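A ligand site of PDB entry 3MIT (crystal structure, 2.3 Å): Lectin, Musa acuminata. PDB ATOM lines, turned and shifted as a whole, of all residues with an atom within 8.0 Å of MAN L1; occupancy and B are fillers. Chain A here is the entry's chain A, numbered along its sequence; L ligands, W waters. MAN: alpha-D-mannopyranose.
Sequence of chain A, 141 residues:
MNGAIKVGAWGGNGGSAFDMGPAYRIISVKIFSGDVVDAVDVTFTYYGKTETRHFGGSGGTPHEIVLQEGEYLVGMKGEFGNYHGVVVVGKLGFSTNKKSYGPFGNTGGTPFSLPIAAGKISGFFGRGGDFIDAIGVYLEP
The side-chain hydroxyl (OG) of Ser 33 lies within hydrogen-bond range of an oxygen (O1) of MAN L2, 3.1 Å away.
O4 of MAN L1 lies within hydrogen-bond range of OD2 of Asp 38 (2.7 Å).
The backbone NH (N) of Gly 60 lies within hydrogen-bond range of an oxygen (O3) of MAN L1, at 2.9 Å.
The backbone carbonyl oxygen (O) of Gly 105 sits at hydrogen-bond distance from an oxygen (O6) of MAN L2 (3.0 Å).
O of Val 36 sits at hydrogen-bond distance from O6 of MAN L1, at 3.1 Å.
The backbone NH (N) of Asp 35 is in hydrogen-bond range of an oxygen (O5) of MAN L1.
The backbone NH of Gly 34 sits at hydrogen-bond distance from an oxygen (O6) of MAN L1, 3.3 Å away.
The backbone NH (N) of Gly 105 sits at hydrogen-bond distance from an oxygen (O6) of MAN L2 (2.7 Å).
O6 of MAN L1 lies within hydrogen-bond range of N of Val 36.
An oxygen (O6) of MAN L2 lies within hydrogen-bond range of the side-chain amide oxygen (OD1) of Asn 106 (2.8 Å).
An oxygen (O1) of MAN L2 lies within hydrogen-bond range of the backbone carbonyl oxygen (O) of Ser 33.
The backbone carbonyl oxygen (O) of Gly 34 lies within hydrogen-bond range of the side-chain amide nitrogen (ND2) of Asn 106 (3.3 Å).
N of Asp 38 is in hydrogen-bond range of O of Phe 32 (2.8 Å).
The backbone NH of Gly 34 sits at hydrogen-bond distance from the side-chain carboxylate of Asp 38.
The backbone carbonyl oxygen (O) of Asp 35 lies within hydrogen-bond range of the backbone NH (N) of Asn 106 (3.1 Å).
OH of Tyr 83 is in hydrogen-bond range of OD2 of Asp 35.
O of Asp 38 sits at hydrogen-bond distance from N of Gly 57 (2.8 Å).
O of Asp 35 is in hydrogen-bond range of OG1 of Thr 107, at 2.5 Å.
Merely in contact with MAN L1: Phe 131 (3.8 Å) and Gly 59 (3.9 Å).
Hydrophobic or aromatic side chains that line MAN L1: Val 36 and Phe 131.
Seven residues have an atom within 4 Å of MAN L1: Gly 34, Asp 35, Val 36, Asp 38, Gly 59, Gly 60 and Phe 131.
Water W1 lies within hydrogen-bond range of O2 of MAN L1 and OG1 of Thr 61.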
ATOM      1  N   PHE A  32      -0.945  27.902  11.598  1.00  0.00           N
ATOM      2  CA  PHE A  32      -1.816  28.491  10.596  1.00  0.00           C
ATOM      3  C   PHE A  32      -3.156  28.838  11.231  1.00  0.00           C
ATOM      4  O   PHE A  32      -3.838  27.963  11.786  1.00  0.00           O
ATOM      5  CB  PHE A  32      -2.036  27.527   9.434  1.00  0.00           C
ATOM      6  CG  PHE A  32      -0.817  27.292   8.592  1.00  0.00           C
ATOM      7  CD1 PHE A  32      -0.649  27.958   7.381  1.00  0.00           C
ATOM      8  CD2 PHE A  32       0.163  26.387   8.992  1.00  0.00           C
ATOM      9  CE1 PHE A  32       0.477  27.743   6.597  1.00  0.00           C
ATOM     10  CE2 PHE A  32       1.290  26.164   8.213  1.00  0.00           C
ATOM     11  CZ  PHE A  32       1.451  26.842   7.006  1.00  0.00           C
ATOM     12  N   SER A  33      -3.542  30.113  11.156  1.00  0.00           N
ATOM     13  CA  SER A  33      -4.806  30.558  11.744  1.00  0.00           C
ATOM     14  C   SER A  33      -5.509  31.676  10.975  1.00  0.00           C
ATOM     15  O   SER A  33      -4.887  32.432  10.220  1.00  0.00           O
ATOM     16  CB  SER A  33      -4.607  30.957  13.220  1.00  0.00           C
ATOM     17  OG  SER A  33      -3.785  32.098  13.347  1.00  0.00           O
ATOM     18  N   GLY A  34      -6.825  31.727  11.150  1.00  0.00           N
ATOM     19  CA  GLY A  34      -7.644  32.847  10.727  1.00  0.00           C
ATOM     20  C   GLY A  34      -8.582  33.129  11.881  1.00  0.00           C
ATOM     21  O   GLY A  34      -8.152  33.566  12.953  1.00  0.00           O
ATOM     22  N   ASP A  35      -9.861  32.849  11.672  1.00  0.00           N
ATOM     23  CA  ASP A  35     -10.871  32.860  12.727  1.00  0.00           C
ATOM     24  C   ASP A  35     -10.548  31.838  13.781  1.00  0.00           C
ATOM     25  O   ASP A  35     -10.861  32.025  14.949  1.00  0.00           O
ATOM     26  CB  ASP A  35     -12.229  32.479  12.144  1.00  0.00           C
ATOM     27  CG  ASP A  35     -12.831  33.554  11.294  1.00  0.00           C
ATOM     28  OD1 ASP A  35     -12.258  34.670  11.247  1.00  0.00           O
ATOM     29  OD2 ASP A  35     -13.878  33.278  10.683  1.00  0.00           O
ATOM     30  N   VAL A  36      -9.935  30.747  13.342  1.00  0.00           N
ATOM     31  CA  VAL A  36      -9.734  29.569  14.160  1.00  0.00           C
ATOM     32  C   VAL A  36      -8.318  29.043  13.913  1.00  0.00           C
ATOM     33  O   VAL A  36      -7.616  29.543  13.047  1.00  0.00           O
ATOM     34  CB  VAL A  36     -10.901  28.554  13.841  1.00  0.00           C
ATOM     35  CG1 VAL A  36     -10.406  27.158  13.481  1.00  0.00           C
ATOM     36  CG2 VAL A  36     -11.947  28.560  14.978  1.00  0.00           C
ATOM     37  N   VAL A  37      -7.870  28.077  14.703  1.00  0.00           N
ATOM     38  CA  VAL A  37      -6.591  27.433  14.421  1.00  0.00           C
ATOM     39  C   VAL A  37      -6.788  26.321  13.380  1.00  0.00           C
ATOM     40  O   VAL A  37      -7.435  25.307  13.651  1.00  0.00           O
ATOM     41  CB  VAL A  37      -5.857  26.937  15.687  1.00  0.00           C
ATOM     42  CG1 VAL A  37      -4.532  26.295  15.333  1.00  0.00           C
ATOM     43  CG2 VAL A  37      -5.656  28.093  16.659  1.00  0.00           C
ATOM     44  N   ASP A  38      -6.236  26.543  12.189  1.00  0.00           N
ATOM     45  CA  ASP A  38      -6.436  25.659  11.066  1.00  0.00           C
ATOM     46  C   ASP A  38      -5.510  24.466  11.119  1.00  0.00           C
ATOM     47  O   ASP A  38      -5.917  23.332  10.822  1.00  0.00           O
ATOM     48  CB  ASP A  38      -6.190  26.421   9.759  1.00  0.00           C
ATOM     49  CG  ASP A  38      -7.256  27.462   9.481  1.00  0.00           C
ATOM     50  OD1 ASP A  38      -7.153  28.590  10.007  1.00  0.00           O
ATOM     51  OD2 ASP A  38      -8.196  27.136   8.733  1.00  0.00           O
ATOM     52  N   ALA A  39      -4.261  24.718  11.514  1.00  0.00           N
ATOM     53  CA  ALA A  39      -3.214  23.743  11.352  1.00  0.00           C
ATOM     54  C   ALA A  39      -1.922  24.138  12.040  1.00  0.00           C
ATOM     55  O   ALA A  39      -1.748  25.284  12.476  1.00  0.00           O
ATOM     56  CB  ALA A  39      -2.957  23.546   9.885  1.00  0.00           C
ATOM     57  N   GLY A  57      -5.745  21.400   8.765  1.00  0.00           N
ATOM     58  CA  GLY A  57      -6.066  21.681   7.366  1.00  0.00           C
ATOM     59  C   GLY A  57      -5.139  22.652   6.657  1.00  0.00           C
ATOM     60  O   GLY A  57      -4.042  22.962   7.131  1.00  0.00           O
ATOM     61  N   SER A  58      -5.591  23.156   5.505  1.00  0.00           N
ATOM     62  CA  SER A  58      -4.743  23.946   4.612  1.00  0.00           C
ATOM     63  C   SER A  58      -5.016  25.451   4.656  1.00  0.00           C
ATOM     64  O   SER A  58      -4.282  26.238   4.035  1.00  0.00           O
ATOM     65  CB  SER A  58      -4.868  23.429   3.175  1.00  0.00           C
ATOM     66  OG  SER A  58      -6.234  23.441   2.786  1.00  0.00           O
ATOM     67  N   GLY A  59      -6.052  25.839   5.379  1.00  0.00           N
ATOM     68  CA  GLY A  59      -6.448  27.249   5.490  1.00  0.00           C
ATOM     69  C   GLY A  59      -5.607  28.034   6.472  1.00  0.00           C
ATOM     70  O   GLY A  59      -4.652  27.507   7.065  1.00  0.00           O
ATOM     71  N   GLY A  60      -5.935  29.305   6.628  1.00  0.00           N
ATOM     72  CA  GLY A  60      -5.286  30.175   7.600  1.00  0.00           C
ATOM     73  C   GLY A  60      -4.021  30.860   7.127  1.00  0.00           C
ATOM     74  O   GLY A  60      -3.487  30.567   6.049  1.00  0.00           O
ATOM     75  N   THR A  61      -3.550  31.789   7.957  1.00  0.00           N
ATOM     76  CA  THR A  61      -2.296  32.516   7.751  1.00  0.00           C
ATOM     77  C   THR A  61      -1.234  31.946   8.701  1.00  0.00           C
ATOM     78  O   THR A  61      -1.515  31.756   9.886  1.00  0.00           O
ATOM     79  CB  THR A  61      -2.519  34.036   8.000  1.00  0.00           C
ATOM     80  OG1 THR A  61      -3.489  34.525   7.070  1.00  0.00           O
ATOM     81  CG2 THR A  61      -1.234  34.829   7.846  1.00  0.00           C
ATOM     82  N   TYR A  83     -17.081  26.137  16.587  1.00  0.00           N
ATOM     83  CA  TYR A  83     -16.995  27.008  15.433  1.00  0.00           C
ATOM     84  C   TYR A  83     -17.753  26.352  14.290  1.00  0.00           C
ATOM     85  O   TYR A  83     -17.229  25.475  13.592  1.00  0.00           O
ATOM     86  CB  TYR A  83     -15.526  27.248  15.042  1.00  0.00           C
ATOM     87  CG  TYR A  83     -15.294  28.141  13.831  1.00  0.00           C
ATOM     88  CD1 TYR A  83     -15.493  29.527  13.915  1.00  0.00           C
ATOM     89  CD2 TYR A  83     -14.841  27.614  12.618  1.00  0.00           C
ATOM     90  CE1 TYR A  83     -15.252  30.346  12.820  1.00  0.00           C
ATOM     91  CE2 TYR A  83     -14.609  28.431  11.519  1.00  0.00           C
ATOM     92  CZ  TYR A  83     -14.816  29.807  11.628  1.00  0.00           C
ATOM     93  OH  TYR A  83     -14.588  30.627  10.537  1.00  0.00           O
ATOM     94  N   VAL A  88     -13.237  23.116  18.082  1.00  0.00           N
ATOM     95  CA  VAL A  88     -11.851  23.203  17.619  1.00  0.00           C
ATOM     96  C   VAL A  88     -11.054  24.222  18.452  1.00  0.00           C
ATOM     97  O   VAL A  88     -11.633  25.012  19.193  1.00  0.00           O
ATOM     98  CB  VAL A  88     -11.747  23.580  16.106  1.00  0.00           C
ATOM     99  CG1 VAL A  88     -12.360  22.503  15.227  1.00  0.00           C
ATOM    100  CG2 VAL A  88     -12.363  24.933  15.808  1.00  0.00           C
ATOM    101  N   VAL A  89      -9.734  24.179  18.314  1.00  0.00           N
ATOM    102  CA  VAL A  89      -8.898  25.224  18.891  1.00  0.00           C
ATOM    103  C   VAL A  89      -9.141  26.539  18.123  1.00  0.00           C
ATOM    104  O   VAL A  89      -8.838  26.666  16.943  1.00  0.00           O
ATOM    105  CB  VAL A  89      -7.398  24.798  18.932  1.00  0.00           C
ATOM    106  CG1 VAL A  89      -6.541  25.888  19.503  1.00  0.00           C
ATOM    107  CG2 VAL A  89      -7.196  23.512  19.763  1.00  0.00           C
ATOM    108  N   GLY A  90      -9.741  27.521  18.800  1.00  0.00           N
ATOM    109  CA  GLY A  90      -9.945  28.844  18.245  1.00  0.00           C
ATOM    110  C   GLY A  90      -8.794  29.811  18.461  1.00  0.00           C
ATOM    111  O   GLY A  90      -8.656  30.776  17.719  1.00  0.00           O
ATOM    112  N   GLY A 105      -5.313  33.058  16.233  1.00  0.00           N
ATOM    113  CA  GLY A 105      -6.720  32.680  16.128  1.00  0.00           C
ATOM    114  C   GLY A 105      -7.566  33.748  16.810  1.00  0.00           C
ATOM    115  O   GLY A 105      -7.106  34.415  17.729  1.00  0.00           O
ATOM    116  N   ASN A 106      -8.809  33.896  16.348  1.00  0.00           N
ATOM    117  CA  ASN A 106      -9.676  34.993  16.774  1.00  0.00           C
ATOM    118  C   ASN A 106     -10.988  34.549  17.425  1.00  0.00           C
ATOM    119  O   ASN A 106     -11.850  35.382  17.682  1.00  0.00           O
ATOM    120  CB  ASN A 106      -9.975  35.942  15.603  1.00  0.00           C
ATOM    121  CG  ASN A 106      -8.708  36.587  15.035  1.00  0.00           C
ATOM    122  OD1 ASN A 106      -7.798  36.964  15.779  1.00  0.00           O
ATOM    123  ND2 ASN A 106      -8.658  36.719  13.715  1.00  0.00           N
ATOM    124  N   THR A 107     -11.134  33.258  17.701  1.00  0.00           N
ATOM    125  CA  THR A 107     -12.379  32.750  18.283  1.00  0.00           C
ATOM    126  C   THR A 107     -12.211  32.300  19.725  1.00  0.00           C
ATOM    127  O   THR A 107     -11.532  31.317  20.032  1.00  0.00           O
ATOM    128  CB  THR A 107     -13.018  31.632  17.420  1.00  0.00           C
ATOM    129  OG1 THR A 107     -13.098  32.066  16.055  1.00  0.00           O
ATOM    130  CG2 THR A 107     -14.422  31.309  17.916  1.00  0.00           C
ATOM    131  N   ASP A 130     -10.337  19.585   9.010  1.00  0.00           N
ATOM    132  CA  ASP A 130     -10.321  20.889   8.350  1.00  0.00           C
ATOM    133  C   ASP A 130      -9.527  21.894   9.200  1.00  0.00           C
ATOM    134  O   ASP A 130      -8.739  22.679   8.666  1.00  0.00           O
ATOM    135  CB  ASP A 130     -11.749  21.392   8.140  1.00  0.00           C
ATOM    136  CG  ASP A 130     -11.867  22.372   6.982  1.00  0.00           C
ATOM    137  OD1 ASP A 130     -10.813  22.748   6.414  1.00  0.00           O
ATOM    138  OD2 ASP A 130     -13.014  22.765   6.609  1.00  0.00           O
ATOM    139  N   PHE A 131      -9.762  21.867  10.504  1.00  0.00           N
ATOM    140  CA  PHE A 131      -9.060  22.713  11.483  1.00  0.00           C
ATOM    141  C   PHE A 131      -8.315  21.845  12.508  1.00  0.00           C
ATOM    142  O   PHE A 131      -8.315  20.629  12.384  1.00  0.00           O
ATOM    143  CB  PHE A 131     -10.045  23.675  12.151  1.00  0.00           C
ATOM    144  CG  PHE A 131     -10.985  24.376  11.181  1.00  0.00           C
ATOM    145  CD1 PHE A 131     -12.376  24.211  11.293  1.00  0.00           C
ATOM    146  CD2 PHE A 131     -10.486  25.183  10.170  1.00  0.00           C
ATOM    147  CE1 PHE A 131     -13.241  24.855  10.410  1.00  0.00           C
ATOM    148  CE2 PHE A 131     -11.347  25.832   9.274  1.00  0.00           C
ATOM    149  CZ  PHE A 131     -12.736  25.658   9.391  1.00  0.00           C
HETATM  150  C1  MAN L   1     -10.738  32.715   7.847  1.00  0.00           C
HETATM  151  C2  MAN L   1      -9.589  32.538   6.856  1.00  0.00           C
HETATM  152  C3  MAN L   1      -9.399  31.069   6.435  1.00  0.00           C
HETATM  153  C4  MAN L   1      -9.467  30.098   7.609  1.00  0.00           C
HETATM  154  C5  MAN L   1     -10.642  30.403   8.549  1.00  0.00           C
HETATM  155  C6  MAN L   1     -10.592  29.556   9.818  1.00  0.00           C
HETATM  156  O1  MAN L   1     -11.975  32.620   7.170  1.00  0.00           O
HETATM  157  O2  MAN L   1      -8.400  33.031   7.433  1.00  0.00           O
HETATM  158  O3  MAN L   1      -8.169  30.913   5.755  1.00  0.00           O
HETATM  159  O4  MAN L   1      -9.592  28.792   7.101  1.00  0.00           O
HETATM  160  O5  MAN L   1     -10.661  31.779   8.907  1.00  0.00           O
HETATM  161  O6  MAN L   1      -9.461  29.898  10.593  1.00  0.00           O
HETATM  162  C1  MAN L   2      -4.859  35.354  11.857  1.00  0.00           C
HETATM  163  C2  MAN L   2      -4.637  36.734  11.243  1.00  0.00           C
HETATM  164  C3  MAN L   2      -3.365  37.390  11.784  1.00  0.00           C
HETATM  165  C4  MAN L   2      -3.352  37.383  13.316  1.00  0.00           C
HETATM  166  C5  MAN L   2      -3.726  36.029  13.909  1.00  0.00           C
HETATM  167  C6  MAN L   2      -3.978  36.183  15.400  1.00  0.00           C
HETATM  168  O1  MAN L   2      -3.871  34.470  11.371  1.00  0.00           O
HETATM  169  O2  MAN L   2      -5.758  37.552  11.494  1.00  0.00           O
HETATM  170  O3  MAN L   2      -3.285  38.707  11.300  1.00  0.00           O
HETATM  171  O4  MAN L   2      -2.077  37.774  13.791  1.00  0.00           O
HETATM  172  O5  MAN L   2      -4.858  35.414  13.285  1.00  0.00           O
HETATM  173  O6  MAN L   2      -5.265  35.699  15.701  1.00  0.00           O
HETATM  174  O   HOH W   1      -6.342  32.967   5.928  1.00  0.00           O
HETATM  175  O   HOH W   2      -8.140  35.781   8.890  1.00  0.00           O
